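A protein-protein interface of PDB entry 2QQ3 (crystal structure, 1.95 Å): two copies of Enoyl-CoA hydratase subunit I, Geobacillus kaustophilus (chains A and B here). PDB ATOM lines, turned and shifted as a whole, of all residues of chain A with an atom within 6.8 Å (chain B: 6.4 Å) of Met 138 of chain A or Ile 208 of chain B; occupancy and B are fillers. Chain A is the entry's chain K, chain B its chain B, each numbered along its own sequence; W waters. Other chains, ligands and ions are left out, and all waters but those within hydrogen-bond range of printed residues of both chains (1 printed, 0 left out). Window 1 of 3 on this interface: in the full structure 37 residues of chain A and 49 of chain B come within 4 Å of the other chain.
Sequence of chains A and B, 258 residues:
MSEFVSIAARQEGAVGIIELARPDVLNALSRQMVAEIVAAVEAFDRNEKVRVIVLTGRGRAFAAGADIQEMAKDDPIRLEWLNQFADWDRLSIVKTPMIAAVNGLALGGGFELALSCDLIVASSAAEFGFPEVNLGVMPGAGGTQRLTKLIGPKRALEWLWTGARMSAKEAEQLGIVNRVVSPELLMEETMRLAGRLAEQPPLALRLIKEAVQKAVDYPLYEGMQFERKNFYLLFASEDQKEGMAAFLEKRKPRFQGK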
ATOM      1  N   PHE A  85      12.055 -33.592 -19.206  1.00  0.00           N
ATOM      2  CA  PHE A  85      10.986 -34.571 -19.107  1.00  0.00           C
ATOM      3  C   PHE A  85      11.443 -35.988 -19.393  1.00  0.00           C
ATOM      4  O   PHE A  85      10.668 -36.937 -19.270  1.00  0.00           O
ATOM      5  CB  PHE A  85       9.824 -34.135 -20.001  1.00  0.00           C
ATOM      6  CG  PHE A  85       9.269 -32.795 -19.614  1.00  0.00           C
ATOM      7  CD1 PHE A  85       8.688 -32.611 -18.360  1.00  0.00           C
ATOM      8  CD2 PHE A  85       9.409 -31.700 -20.452  1.00  0.00           C
ATOM      9  CE1 PHE A  85       8.260 -31.345 -17.944  1.00  0.00           C
ATOM     10  CE2 PHE A  85       8.987 -30.431 -20.050  1.00  0.00           C
ATOM     11  CZ  PHE A  85       8.411 -30.254 -18.791  1.00  0.00           C
ATOM     12  N   GLU A 112       0.758 -34.432 -11.874  1.00  0.00           N
ATOM     13  CA  GLU A 112       1.371 -35.313 -12.863  1.00  0.00           C
ATOM     14  C   GLU A 112       2.120 -36.467 -12.217  1.00  0.00           C
ATOM     15  O   GLU A 112       2.156 -37.574 -12.764  1.00  0.00           O
ATOM     16  CB  GLU A 112       2.290 -34.503 -13.779  1.00  0.00           C
ATOM     17  CG  GLU A 112       1.502 -33.529 -14.651  1.00  0.00           C
ATOM     18  CD  GLU A 112       2.367 -32.527 -15.376  1.00  0.00           C
ATOM     19  OE1 GLU A 112       3.176 -31.852 -14.703  1.00  0.00           O
ATOM     20  OE2 GLU A 112       2.226 -32.405 -16.614  1.00  0.00           O
ATOM     21  N   PHE A 130      -4.258 -28.143 -12.344  1.00  0.00           N
ATOM     22  CA  PHE A 130      -3.169 -27.732 -13.228  1.00  0.00           C
ATOM     23  C   PHE A 130      -3.204 -26.216 -13.372  1.00  0.00           C
ATOM     24  O   PHE A 130      -3.818 -25.679 -14.297  1.00  0.00           O
ATOM     25  CB  PHE A 130      -3.314 -28.386 -14.609  1.00  0.00           C
ATOM     26  CG  PHE A 130      -3.005 -29.854 -14.615  1.00  0.00           C
ATOM     27  CD1 PHE A 130      -1.724 -30.309 -14.306  1.00  0.00           C
ATOM     28  CD2 PHE A 130      -3.994 -30.785 -14.907  1.00  0.00           C
ATOM     29  CE1 PHE A 130      -1.435 -31.673 -14.288  1.00  0.00           C
ATOM     30  CE2 PHE A 130      -3.716 -32.153 -14.891  1.00  0.00           C
ATOM     31  CZ  PHE A 130      -2.436 -32.597 -14.581  1.00  0.00           C
ATOM     32  N   GLU A 132      -0.867 -24.298 -14.248  1.00  0.00           N
ATOM     33  CA  GLU A 132       0.059 -23.856 -15.287  1.00  0.00           C
ATOM     34  C   GLU A 132      -0.475 -22.779 -16.236  1.00  0.00           C
ATOM     35  O   GLU A 132       0.228 -21.812 -16.530  1.00  0.00           O
ATOM     36  CB  GLU A 132       0.547 -25.053 -16.120  1.00  0.00           C
ATOM     37  CG  GLU A 132       1.596 -25.909 -15.425  1.00  0.00           C
ATOM     38  CD  GLU A 132       0.996 -27.043 -14.621  1.00  0.00           C
ATOM     39  OE1 GLU A 132      -0.192 -26.944 -14.232  1.00  0.00           O
ATOM     40  OE2 GLU A 132       1.721 -28.030 -14.371  1.00  0.00           O
ATOM     41  N   VAL A 133      -1.703 -22.947 -16.726  1.00  0.00           N
ATOM     42  CA  VAL A 133      -2.273 -21.968 -17.647  1.00  0.00           C
ATOM     43  C   VAL A 133      -2.236 -20.557 -17.068  1.00  0.00           C
ATOM     44  O   VAL A 133      -2.007 -19.586 -17.789  1.00  0.00           O
ATOM     45  CB  VAL A 133      -3.743 -22.319 -18.024  1.00  0.00           C
ATOM     46  CG1 VAL A 133      -4.598 -22.426 -16.773  1.00  0.00           C
ATOM     47  CG2 VAL A 133      -4.311 -21.259 -18.958  1.00  0.00           C
ATOM     48  N   LEU A 135      -0.042 -19.332 -15.327  1.00  0.00           N
ATOM     49  CA  LEU A 135       1.345 -18.880 -15.285  1.00  0.00           C
ATOM     50  C   LEU A 135       1.820 -18.588 -16.704  1.00  0.00           C
ATOM     51  O   LEU A 135       2.986 -18.270 -16.927  1.00  0.00           O
ATOM     52  CB  LEU A 135       2.241 -19.947 -14.660  1.00  0.00           C
ATOM     53  CG  LEU A 135       2.195 -20.028 -13.134  1.00  0.00           C
ATOM     54  CD1 LEU A 135       3.007 -21.210 -12.633  1.00  0.00           C
ATOM     55  CD2 LEU A 135       2.744 -18.742 -12.577  1.00  0.00           C
ATOM     56  N   GLY A 136       0.901 -18.696 -17.659  1.00  0.00           N
ATOM     57  CA  GLY A 136       1.240 -18.446 -19.048  1.00  0.00           C
ATOM     58  C   GLY A 136       1.751 -19.678 -19.778  1.00  0.00           C
ATOM     59  O   GLY A 136       2.133 -19.593 -20.946  1.00  0.00           O
ATOM     60  N   VAL A 137       1.764 -20.826 -19.104  1.00  0.00           N
ATOM     61  CA  VAL A 137       2.245 -22.052 -19.735  1.00  0.00           C
ATOM     62  C   VAL A 137       1.208 -23.171 -19.721  1.00  0.00           C
ATOM     63  O   VAL A 137       0.011 -22.915 -19.827  1.00  0.00           O
ATOM     64  CB  VAL A 137       3.559 -22.549 -19.078  1.00  0.00           C
ATOM     65  CG1 VAL A 137       4.658 -21.526 -19.296  1.00  0.00           C
ATOM     66  CG2 VAL A 137       3.352 -22.801 -17.586  1.00  0.00           C
ATOM     67  N   MET A 138       1.666 -24.409 -19.582  1.00  0.00           N
ATOM     68  CA  MET A 138       0.760 -25.551 -19.590  1.00  0.00           C
ATOM     69  C   MET A 138       1.476 -26.729 -18.955  1.00  0.00           C
ATOM     70  O   MET A 138       2.677 -26.662 -18.721  1.00  0.00           O
ATOM     71  CB  MET A 138       0.407 -25.907 -21.042  1.00  0.00           C
ATOM     72  CG  MET A 138       1.625 -26.373 -21.850  1.00  0.00           C
ATOM     73  SD  MET A 138       1.291 -26.684 -23.607  1.00  0.00           S
ATOM     74  CE  MET A 138       0.670 -28.401 -23.517  1.00  0.00           C
ATOM     75  N   PRO A 139       0.745 -27.816 -18.643  1.00  0.00           N
ATOM     76  CA  PRO A 139       1.411 -28.980 -18.044  1.00  0.00           C
ATOM     77  C   PRO A 139       2.395 -29.518 -19.083  1.00  0.00           C
ATOM     78  O   PRO A 139       2.090 -29.523 -20.278  1.00  0.00           O
ATOM     79  CB  PRO A 139       0.255 -29.953 -17.798  1.00  0.00           C
ATOM     80  CG  PRO A 139      -0.912 -29.028 -17.542  1.00  0.00           C
ATOM     81  CD  PRO A 139      -0.720 -27.974 -18.614  1.00  0.00           C
ATOM     82  N   GLY A 140       3.567 -29.964 -18.639  1.00  0.00           N
ATOM     83  CA  GLY A 140       4.546 -30.478 -19.578  1.00  0.00           C
ATOM     84  C   GLY A 140       5.056 -31.874 -19.268  1.00  0.00           C
ATOM     85  O   GLY A 140       5.889 -32.407 -20.003  1.00  0.00           O
ATOM     86  N   ALA A 141       4.563 -32.469 -18.186  1.00  0.00           N
ATOM     87  CA  ALA A 141       4.989 -33.809 -17.800  1.00  0.00           C
ATOM     88  C   ALA A 141       3.864 -34.848 -17.912  1.00  0.00           C
ATOM     89  O   ALA A 141       3.667 -35.678 -17.019  1.00  0.00           O
ATOM     90  CB  ALA A 141       5.554 -33.791 -16.378  1.00  0.00           C
ATOM     91  N   THR A 144      -1.607 -33.065 -19.596  1.00  0.00           N
ATOM     92  CA  THR A 144      -2.663 -32.929 -20.596  1.00  0.00           C
ATOM     93  C   THR A 144      -3.030 -34.273 -21.218  1.00  0.00           C
ATOM     94  O   THR A 144      -4.162 -34.472 -21.651  1.00  0.00           O
ATOM     95  CB  THR A 144      -2.254 -31.969 -21.744  1.00  0.00           C
ATOM     96  OG1 THR A 144      -1.125 -32.505 -22.447  1.00  0.00           O
ATOM     97  CG2 THR A 144      -1.913 -30.591 -21.195  1.00  0.00           C
ATOM     98  N   GLN A 145      -2.073 -35.194 -21.253  1.00  0.00           N
ATOM     99  CA  GLN A 145      -2.303 -36.504 -21.849  1.00  0.00           C
ATOM    100  C   GLN A 145      -3.018 -37.471 -20.914  1.00  0.00           C
ATOM    101  O   GLN A 145      -4.024 -38.069 -21.287  1.00  0.00           O
ATOM    102  CB  GLN A 145      -0.971 -37.111 -22.304  1.00  0.00           C
ATOM    103  CG  GLN A 145      -0.162 -36.189 -23.201  1.00  0.00           C
ATOM    104  CD  GLN A 145      -0.943 -35.728 -24.409  1.00  0.00           C
ATOM    105  OE1 GLN A 145      -1.308 -34.554 -24.519  1.00  0.00           O
ATOM    106  NE2 GLN A 145      -1.216 -36.653 -25.324  1.00  0.00           N
ATOM    107  N   THR A 148      -6.743 -36.233 -19.979  1.00  0.00           N
ATOM    108  CA  THR A 148      -7.676 -36.389 -21.090  1.00  0.00           C
ATOM    109  C   THR A 148      -8.041 -37.861 -21.290  1.00  0.00           C
ATOM    110  O   THR A 148      -9.200 -38.195 -21.522  1.00  0.00           O
ATOM    111  CB  THR A 148      -7.099 -35.827 -22.401  1.00  0.00           C
ATOM    112  OG1 THR A 148      -6.903 -34.414 -22.268  1.00  0.00           O
ATOM    113  CG2 THR A 148      -8.055 -36.087 -23.566  1.00  0.00           C
ATOM    114  N   ALA A 156     -11.560 -32.480 -19.600  1.00  0.00           N
ATOM    115  CA  ALA A 156     -10.131 -32.183 -19.486  1.00  0.00           C
ATOM    116  C   ALA A 156      -9.820 -30.716 -19.784  1.00  0.00           C
ATOM    117  O   ALA A 156      -9.110 -30.057 -19.021  1.00  0.00           O
ATOM    118  CB  ALA A 156      -9.329 -33.079 -20.425  1.00  0.00           C
ATOM    119  N   LEU A 157     -10.346 -30.210 -20.895  1.00  0.00           N
ATOM    120  CA  LEU A 157     -10.111 -28.824 -21.294  1.00  0.00           C
ATOM    121  C   LEU A 157     -10.625 -27.822 -20.275  1.00  0.00           C
ATOM    122  O   LEU A 157     -10.012 -26.778 -20.068  1.00  0.00           O
ATOM    123  CB  LEU A 157     -10.757 -28.537 -22.651  1.00  0.00           C
ATOM    124  CG  LEU A 157      -9.941 -28.930 -23.883  1.00  0.00           C
ATOM    125  CD1 LEU A 157     -10.762 -28.683 -25.136  1.00  0.00           C
ATOM    126  CD2 LEU A 157      -8.644 -28.119 -23.919  1.00  0.00           C
ATOM    127  N   LEU A 160      -7.977 -27.870 -17.513  1.00  0.00           N
ATOM    128  CA  LEU A 160      -6.701 -27.377 -18.027  1.00  0.00           C
ATOM    129  C   LEU A 160      -6.720 -25.909 -18.442  1.00  0.00           C
ATOM    130  O   LEU A 160      -5.713 -25.214 -18.321  1.00  0.00           O
ATOM    131  CB  LEU A 160      -6.253 -28.238 -19.210  1.00  0.00           C
ATOM    132  CG  LEU A 160      -5.910 -29.681 -18.826  1.00  0.00           C
ATOM    133  CD1 LEU A 160      -6.002 -30.577 -20.045  1.00  0.00           C
ATOM    134  CD2 LEU A 160      -4.519 -29.729 -18.195  1.00  0.00           C
ATOM    135  N   TRP A 161      -7.861 -25.438 -18.940  1.00  0.00           N
ATOM    136  CA  TRP A 161      -7.980 -24.049 -19.376  1.00  0.00           C
ATOM    137  C   TRP A 161      -8.211 -23.060 -18.231  1.00  0.00           C
ATOM    138  O   TRP A 161      -7.850 -21.889 -18.337  1.00  0.00           O
ATOM    139  CB  TRP A 161      -9.124 -23.905 -20.381  1.00  0.00           C
ATOM    140  CG  TRP A 161      -8.760 -24.146 -21.823  1.00  0.00           C
ATOM    141  CD1 TRP A 161      -7.509 -24.317 -22.347  1.00  0.00           C
ATOM    142  CD2 TRP A 161      -9.667 -24.163 -22.933  1.00  0.00           C
ATOM    143  NE1 TRP A 161      -7.584 -24.431 -23.716  1.00  0.00           N
ATOM    144  CE2 TRP A 161      -8.897 -24.339 -24.101  1.00  0.00           C
ATOM    145  CE3 TRP A 161     -11.061 -24.040 -23.050  1.00  0.00           C
ATOM    146  CZ2 TRP A 161      -9.471 -24.398 -25.376  1.00  0.00           C
ATOM    147  CZ3 TRP A 161     -11.634 -24.098 -24.319  1.00  0.00           C
ATOM    148  CH2 TRP A 161     -10.837 -24.276 -25.464  1.00  0.00           C
ATOM    149  N   LEU B 203      -1.971 -17.965 -25.981  1.00  0.00           N
ATOM    150  CA  LEU B 203      -1.081 -19.018 -26.464  1.00  0.00           C
ATOM    151  C   LEU B 203      -1.259 -20.307 -25.682  1.00  0.00           C
ATOM    152  O   LEU B 203      -1.273 -21.396 -26.264  1.00  0.00           O
ATOM    153  CB  LEU B 203       0.384 -18.563 -26.392  1.00  0.00           C
ATOM    154  CG  LEU B 203       0.826 -17.670 -27.553  1.00  0.00           C
ATOM    155  CD1 LEU B 203       2.217 -17.103 -27.280  1.00  0.00           C
ATOM    156  CD2 LEU B 203       0.809 -18.487 -28.845  1.00  0.00           C
ATOM    157  N   ALA B 204      -1.391 -20.184 -24.364  1.00  0.00           N
ATOM    158  CA  ALA B 204      -1.567 -21.350 -23.510  1.00  0.00           C
ATOM    159  C   ALA B 204      -2.853 -22.104 -23.869  1.00  0.00           C
ATOM    160  O   ALA B 204      -2.847 -23.330 -23.964  1.00  0.00           O
ATOM    161  CB  ALA B 204      -1.591 -20.933 -22.044  1.00  0.00           C
ATOM    162  N   LEU B 205      -3.952 -21.378 -24.060  1.00  0.00           N
ATOM    163  CA  LEU B 205      -5.217 -22.018 -24.429  1.00  0.00           C
ATOM    164  C   LEU B 205      -5.054 -22.760 -25.754  1.00  0.00           C
ATOM    165  O   LEU B 205      -5.503 -23.897 -25.914  1.00  0.00           O
ATOM    166  CB  LEU B 205      -6.341 -20.986 -24.585  1.00  0.00           C
ATOM    167  CG  LEU B 205      -6.784 -20.163 -23.368  1.00  0.00           C
ATOM    168  CD1 LEU B 205      -8.189 -19.621 -23.631  1.00  0.00           C
ATOM    169  CD2 LEU B 205      -6.791 -21.013 -22.116  1.00  0.00           C
ATOM    170  N   ARG B 206      -4.417 -22.084 -26.701  1.00  0.00           N
ATOM    171  CA  ARG B 206      -4.173 -22.620 -28.028  1.00  0.00           C
ATOM    172  C   ARG B 206      -3.396 -23.940 -27.969  1.00  0.00           C
ATOM    173  O   ARG B 206      -3.853 -24.960 -28.486  1.00  0.00           O
ATOM    174  CB  ARG B 206      -3.382 -21.587 -28.839  1.00  0.00           C
ATOM    175  CG  ARG B 206      -3.194 -21.902 -30.323  1.00  0.00           C
ATOM    176  CD  ARG B 206      -2.226 -20.881 -30.928  1.00  0.00           C
ATOM    177  NE  ARG B 206      -2.020 -20.996 -32.371  1.00  0.00           N
ATOM    178  CZ  ARG B 206      -2.932 -20.702 -33.294  1.00  0.00           C
ATOM    179  NH1 ARG B 206      -4.139 -20.281 -32.939  1.00  0.00           N
ATOM    180  NH2 ARG B 206      -2.620 -20.792 -34.581  1.00  0.00           N
ATOM    181  N   LEU B 207      -2.227 -23.916 -27.334  1.00  0.00           N
ATOM    182  CA  LEU B 207      -1.388 -25.109 -27.249  1.00  0.00           C
ATOM    183  C   LEU B 207      -1.946 -26.202 -26.348  1.00  0.00           C
ATOM    184  O   LEU B 207      -1.706 -27.384 -26.583  1.00  0.00           O
ATOM    185  CB  LEU B 207       0.033 -24.720 -26.830  1.00  0.00           C
ATOM    186  CG  LEU B 207       0.942 -24.320 -28.009  1.00  0.00           C
ATOM    187  CD1 LEU B 207       0.185 -23.462 -29.015  1.00  0.00           C
ATOM    188  CD2 LEU B 207       2.162 -23.585 -27.492  1.00  0.00           C
ATOM    189  N   ILE B 208      -2.698 -25.817 -25.323  1.00  0.00           N
ATOM    190  CA  ILE B 208      -3.307 -26.811 -24.443  1.00  0.00           C
ATOM    191  C   ILE B 208      -4.393 -27.521 -25.243  1.00  0.00           C
ATOM    192  O   ILE B 208      -4.591 -28.731 -25.116  1.00  0.00           O
ATOM    193  CB  ILE B 208      -3.943 -26.153 -23.187  1.00  0.00           C
ATOM    194  CG1 ILE B 208      -2.833 -25.725 -22.222  1.00  0.00           C
ATOM    195  CG2 ILE B 208      -4.907 -27.130 -22.512  1.00  0.00           C
ATOM    196  CD1 ILE B 208      -3.306 -24.954 -21.008  1.00  0.00           C
ATOM    197  N   LYS B 209      -5.101 -26.762 -26.075  1.00  0.00           N
ATOM    198  CA  LYS B 209      -6.154 -27.351 -26.885  1.00  0.00           C
ATOM    199  C   LYS B 209      -5.547 -28.376 -27.845  1.00  0.00           C
ATOM    200  O   LYS B 209      -6.114 -29.446 -28.038  1.00  0.00           O
ATOM    201  CB  LYS B 209      -6.912 -26.274 -27.671  1.00  0.00           C
ATOM    202  CG  LYS B 209      -7.923 -26.852 -28.653  1.00  0.00           C
ATOM    203  CD  LYS B 209      -8.754 -25.772 -29.324  1.00  0.00           C
ATOM    204  CE  LYS B 209      -9.649 -26.376 -30.398  1.00  0.00           C
ATOM    205  NZ  LYS B 209     -10.511 -25.363 -31.064  1.00  0.00           N
ATOM    206  N   GLU B 210      -4.399 -28.054 -28.439  1.00  0.00           N
ATOM    207  CA  GLU B 210      -3.761 -28.991 -29.354  1.00  0.00           C
ATOM    208  C   GLU B 210      -3.346 -30.257 -28.629  1.00  0.00           C
ATOM    209  O   GLU B 210      -3.532 -31.359 -29.150  1.00  0.00           O
ATOM    210  CB  GLU B 210      -2.522 -28.384 -30.005  1.00  0.00           C
ATOM    211  CG  GLU B 210      -2.779 -27.210 -30.917  1.00  0.00           C
ATOM    212  CD  GLU B 210      -1.521 -26.781 -31.654  1.00  0.00           C
ATOM    213  OE1 GLU B 210      -0.440 -26.732 -31.018  1.00  0.00           O
ATOM    214  OE2 GLU B 210      -1.609 -26.489 -32.864  1.00  0.00           O
ATOM    215  N   ALA B 211      -2.778 -30.101 -27.433  1.00  0.00           N
ATOM    216  CA  ALA B 211      -2.333 -31.249 -26.648  1.00  0.00           C
ATOM    217  C   ALA B 211      -3.489 -32.183 -26.323  1.00  0.00           C
ATOM    218  O   ALA B 211      -3.368 -33.396 -26.468  1.00  0.00           O
ATOM    219  CB  ALA B 211      -1.657 -30.789 -25.353  1.00  0.00           C
ATOM    220  N   VAL B 212      -4.605 -31.611 -25.876  1.00  0.00           N
ATOM    221  CA  VAL B 212      -5.782 -32.402 -25.536  1.00  0.00           C
ATOM    222  C   VAL B 212      -6.264 -33.177 -26.760  1.00  0.00           C
ATOM    223  O   VAL B 212      -6.648 -34.343 -26.661  1.00  0.00           O
ATOM    224  CB  VAL B 212      -6.915 -31.497 -24.997  1.00  0.00           C
ATOM    225  CG1 VAL B 212      -8.218 -32.294 -24.848  1.00  0.00           C
ATOM    226  CG2 VAL B 212      -6.498 -30.915 -23.649  1.00  0.00           C
ATOM    227  N   GLN B 213      -6.226 -32.534 -27.921  1.00  0.00           N
ATOM    228  CA  GLN B 213      -6.653 -33.194 -29.150  1.00  0.00           C
ATOM    229  C   GLN B 213      -5.742 -34.371 -29.496  1.00  0.00           C
ATOM    230  O   GLN B 213      -6.208 -35.383 -30.015  1.00  0.00           O
ATOM    231  CB  GLN B 213      -6.693 -32.191 -30.303  1.00  0.00           C
ATOM    232  CG  GLN B 213      -7.655 -31.036 -30.049  1.00  0.00           C
ATOM    233  CD  GLN B 213      -7.784 -30.099 -31.233  1.00  0.00           C
ATOM    234  OE1 GLN B 213      -6.786 -29.607 -31.765  1.00  0.00           O
ATOM    235  NE2 GLN B 213      -9.017 -29.842 -31.651  1.00  0.00           N
ATOM    236  N   PHE B 226       4.659 -34.669 -27.930  1.00  0.00           N
ATOM    237  CA  PHE B 226       4.070 -33.497 -28.565  1.00  0.00           C
ATOM    238  C   PHE B 226       3.822 -32.420 -27.517  1.00  0.00           C
ATOM    239  O   PHE B 226       4.079 -31.236 -27.732  1.00  0.00           O
ATOM    240  CB  PHE B 226       2.737 -33.872 -29.210  1.00  0.00           C
ATOM    241  CG  PHE B 226       2.041 -32.718 -29.859  1.00  0.00           C
ATOM    242  CD1 PHE B 226       2.335 -32.360 -31.166  1.00  0.00           C
ATOM    243  CD2 PHE B 226       1.105 -31.969 -29.152  1.00  0.00           C
ATOM    244  CE1 PHE B 226       1.707 -31.270 -31.767  1.00  0.00           C
ATOM    245  CE2 PHE B 226       0.472 -30.876 -29.743  1.00  0.00           C
ATOM    246  CZ  PHE B 226       0.775 -30.527 -31.053  1.00  0.00           C
ATOM    247  N   GLU B 227       3.298 -32.853 -26.382  1.00  0.00           N
ATOM    248  CA  GLU B 227       2.992 -31.961 -25.281  1.00  0.00           C
ATOM    249  C   GLU B 227       4.195 -31.115 -24.869  1.00  0.00           C
ATOM    250  O   GLU B 227       4.100 -29.888 -24.798  1.00  0.00           O
ATOM    251  CB  GLU B 227       2.513 -32.784 -24.085  1.00  0.00           C
ATOM    252  CG  GLU B 227       2.188 -31.976 -22.849  1.00  0.00           C
ATOM    253  CD  GLU B 227       2.006 -32.864 -21.647  1.00  0.00           C
ATOM    254  OE1 GLU B 227       2.994 -33.529 -21.261  1.00  0.00           O
ATOM    255  OE2 GLU B 227       0.884 -32.912 -21.093  1.00  0.00           O
ATOM    256  N   ARG B 228       5.325 -31.766 -24.599  1.00  0.00           N
ATOM    257  CA  ARG B 228       6.510 -31.030 -24.170  1.00  0.00           C
ATOM    258  C   ARG B 228       7.036 -30.066 -25.231  1.00  0.00           C
ATOM    259  O   ARG B 228       7.592 -29.026 -24.893  1.00  0.00           O
ATOM    260  CB  ARG B 228       7.615 -31.991 -23.710  1.00  0.00           C
ATOM    261  CG  ARG B 228       8.183 -32.893 -24.783  1.00  0.00           C
ATOM    262  CD  ARG B 228       8.995 -34.015 -24.140  1.00  0.00           C
ATOM    263  NE  ARG B 228       8.198 -34.791 -23.195  1.00  0.00           N
ATOM    264  CZ  ARG B 228       8.584 -35.942 -22.644  1.00  0.00           C
ATOM    265  NH1 ARG B 228       9.768 -36.461 -22.944  1.00  0.00           N
ATOM    266  NH2 ARG B 228       7.782 -36.574 -21.791  1.00  0.00           N
ATOM    267  N   ASN B 230       5.211 -28.307 -27.134  1.00  0.00           N
ATOM    268  CA  ASN B 230       4.373 -27.119 -26.975  1.00  0.00           C
ATOM    269  C   ASN B 230       4.827 -26.379 -25.714  1.00  0.00           C
ATOM    270  O   ASN B 230       4.856 -25.150 -25.684  1.00  0.00           O
ATOM    271  CB  ASN B 230       2.888 -27.499 -26.880  1.00  0.00           C
ATOM    272  CG  ASN B 230       2.191 -27.454 -28.239  1.00  0.00           C
ATOM    273  OD1 ASN B 230       2.817 -27.147 -29.251  1.00  0.00           O
ATOM    274  ND2 ASN B 230       0.890 -27.752 -28.262  1.00  0.00           N
ATOM    275  N   PHE B 231       5.192 -27.141 -24.686  1.00  0.00           N
ATOM    276  CA  PHE B 231       5.671 -26.569 -23.430  1.00  0.00           C
ATOM    277  C   PHE B 231       6.853 -25.656 -23.766  1.00  0.00           C
ATOM    278  O   PHE B 231       6.867 -24.493 -23.371  1.00  0.00           O
ATOM    279  CB  PHE B 231       6.133 -27.682 -22.482  1.00  0.00           C
ATOM    280  CG  PHE B 231       6.511 -27.205 -21.096  1.00  0.00           C
ATOM    281  CD1 PHE B 231       5.531 -26.890 -20.157  1.00  0.00           C
ATOM    282  CD2 PHE B 231       7.848 -27.103 -20.722  1.00  0.00           C
ATOM    283  CE1 PHE B 231       5.879 -26.485 -18.860  1.00  0.00           C
ATOM    284  CE2 PHE B 231       8.206 -26.698 -19.428  1.00  0.00           C
ATOM    285  CZ  PHE B 231       7.216 -26.389 -18.496  1.00  0.00           C
ATOM    286  N   LEU B 234       6.084 -22.261 -25.457  1.00  0.00           N
ATOM    287  CA  LEU B 234       5.503 -21.237 -24.600  1.00  0.00           C
ATOM    288  C   LEU B 234       6.575 -20.360 -23.951  1.00  0.00           C
ATOM    289  O   LEU B 234       6.321 -19.199 -23.636  1.00  0.00           O
ATOM    290  CB  LEU B 234       4.610 -21.888 -23.536  1.00  0.00           C
ATOM    291  CG  LEU B 234       3.330 -22.490 -24.138  1.00  0.00           C
ATOM    292  CD1 LEU B 234       2.616 -23.384 -23.128  1.00  0.00           C
ATOM    293  CD2 LEU B 234       2.421 -21.363 -24.609  1.00  0.00           C
HETATM  294  O   HOH W   1       5.712 -34.521 -21.601  1.00  0.00           O
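The side-chain amide oxygen of Gln 145 of chain A lies close to the backbone carbonyl oxygen of Ala 211 of chain B, at 3.1 Å. The backbone carbonyl oxygen (O) of Gly 140 of chain A sits close to the side-chain carboxylate (OE1) of Glu 227 of chain B, at 3.3 Å. The indole nitrogen (NE1) of Trp 161 of chain A is in hydrogen-bond range of the backbone carbonyl oxygen (O) of Leu 205 of chain B (3.1 Å). The side-chain hydroxyl (OG1) of Thr 144 of chain A sits at hydrogen-bond distance from the side-chain carboxylate (OE2) of Glu 227 of chain B.
OG1 of Thr 148 of chain A sits at hydrogen-bond distance from O of Thr 144 of chain A (2.8 Å). The side-chain carboxylate (OE1) of Glu 210 of chain B is in hydrogen-bond range of the side-chain amide nitrogen (ND2) of Asn 230 of chain B (3.2 Å). The side-chain carboxylate (OE2) of Glu 112 of chain A lies within hydrogen-bond range of the backbone NH (N) of Ala 141 of chain A (2.8 Å). The side-chain hydroxyl (OG1) of Thr 144 of chain A sits at hydrogen-bond distance from the side-chain amide oxygen (OE1) of Gln 145 of chain A, at 2.9 Å. N of Val 137 of chain A is in hydrogen-bond range of O of Glu 132 of chain A (3.2 Å).
Ile 208 of chain B touches Met 138 of chain A. CB of Asn 230 of chain B touches SD of Met 138 of chain A (3.7 Å). Met 138 of chain A touches Phe 231 of chain B (O to CD1, 3.2 Å). N of Ala 141 of chain A touches OE1 of Glu 227 of chain B (3.6 Å). CB of Ala 211 of chain B touches OG1 of Thr 144 of chain A (3.4 Å). Leu 157 of chain A touches Lys 209 of chain B (CD2 to CA, 3.9 Å). CG2 of Val 212 of chain B touches CD2 of Leu 157 of chain A (3.5 Å). Ile 208 of chain B touches Leu 160 of chain A (CD1 to O, 3.6 Å). CG2 of Val 212 of chain B touches CD1 of Leu 160 of chain A, 3.7 Å away. Trp 161 of chain A touches Lys 209 of chain B (CZ2 to CB, 3.9 Å).
Printed residues of chain B within 4 Å of Met 138 of chain A: Leu 207, Ile 208, Ala 211, Glu 227, Asn 230, Phe 231 and Leu 234. Printed residues of chain A within 4 Å of Ile 208 of chain B: Met 138, Leu 160 and Trp 161. Printed residues of chain A within 4 Å of Glu 227 of chain B: Met 138 (3.9 Å), Pro 139 (3.6 Å), Gly 140 (3.3 Å), Ala 141 (3.6 Å), Thr 144 (2.5 Å) and Gln 145 (3.7 Å). Of the printed residues of chain A, Leu 207 of chain B touches Met 138 (3.98 Å). Of the printed residues of chain B, Val 137 of chain A touches Ala 204 and Leu 234. Of the printed residues of chain B, Ala 141 of chain A touches Glu 227 (3.6 Å). Leu 203 of chain B touches none of the printed residues of chain A. Glu 112 of chain A touches none of the printed residues of chain B. The nearest residue of chain B that does not touch Met 138 of chain A is Ala 204 of chain B (5.1 Å). The nearest printed residue of chain B that does not touch Thr 144 of chain A is Val 212 of chain B (4.7 Å).
Of the 19 printed residues of chain A, 12 touch a printed residue of chain B. Printed residues of chain A that touch a printed residue of chain B: Phe 85, Val 137, Met 138, Pro 139, Gly 140, Ala 141, Thr 144, Gln 145, Thr 148, Leu 157, Leu 160 and Trp 161. Hydrophobic or aromatic side chains of chain B that line the printed part of chain A: Ala 204, Leu 205, Leu 207, Ile 208, Ala 211, Val 212, Phe 231 and Leu 234.
No position is printed for both chains. Of the 27 pairs that touch across the chains among the printed residues, none has its exchanged pair printed and touching as well.
Water W1 lies within hydrogen-bond range of the backbone carbonyl oxygen (O) of Gly 140 of chain A, the side-chain carboxylate (OE1) of Glu 227 of chain B and the guanidinium group (NH2) of Arg 228 of chain B.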
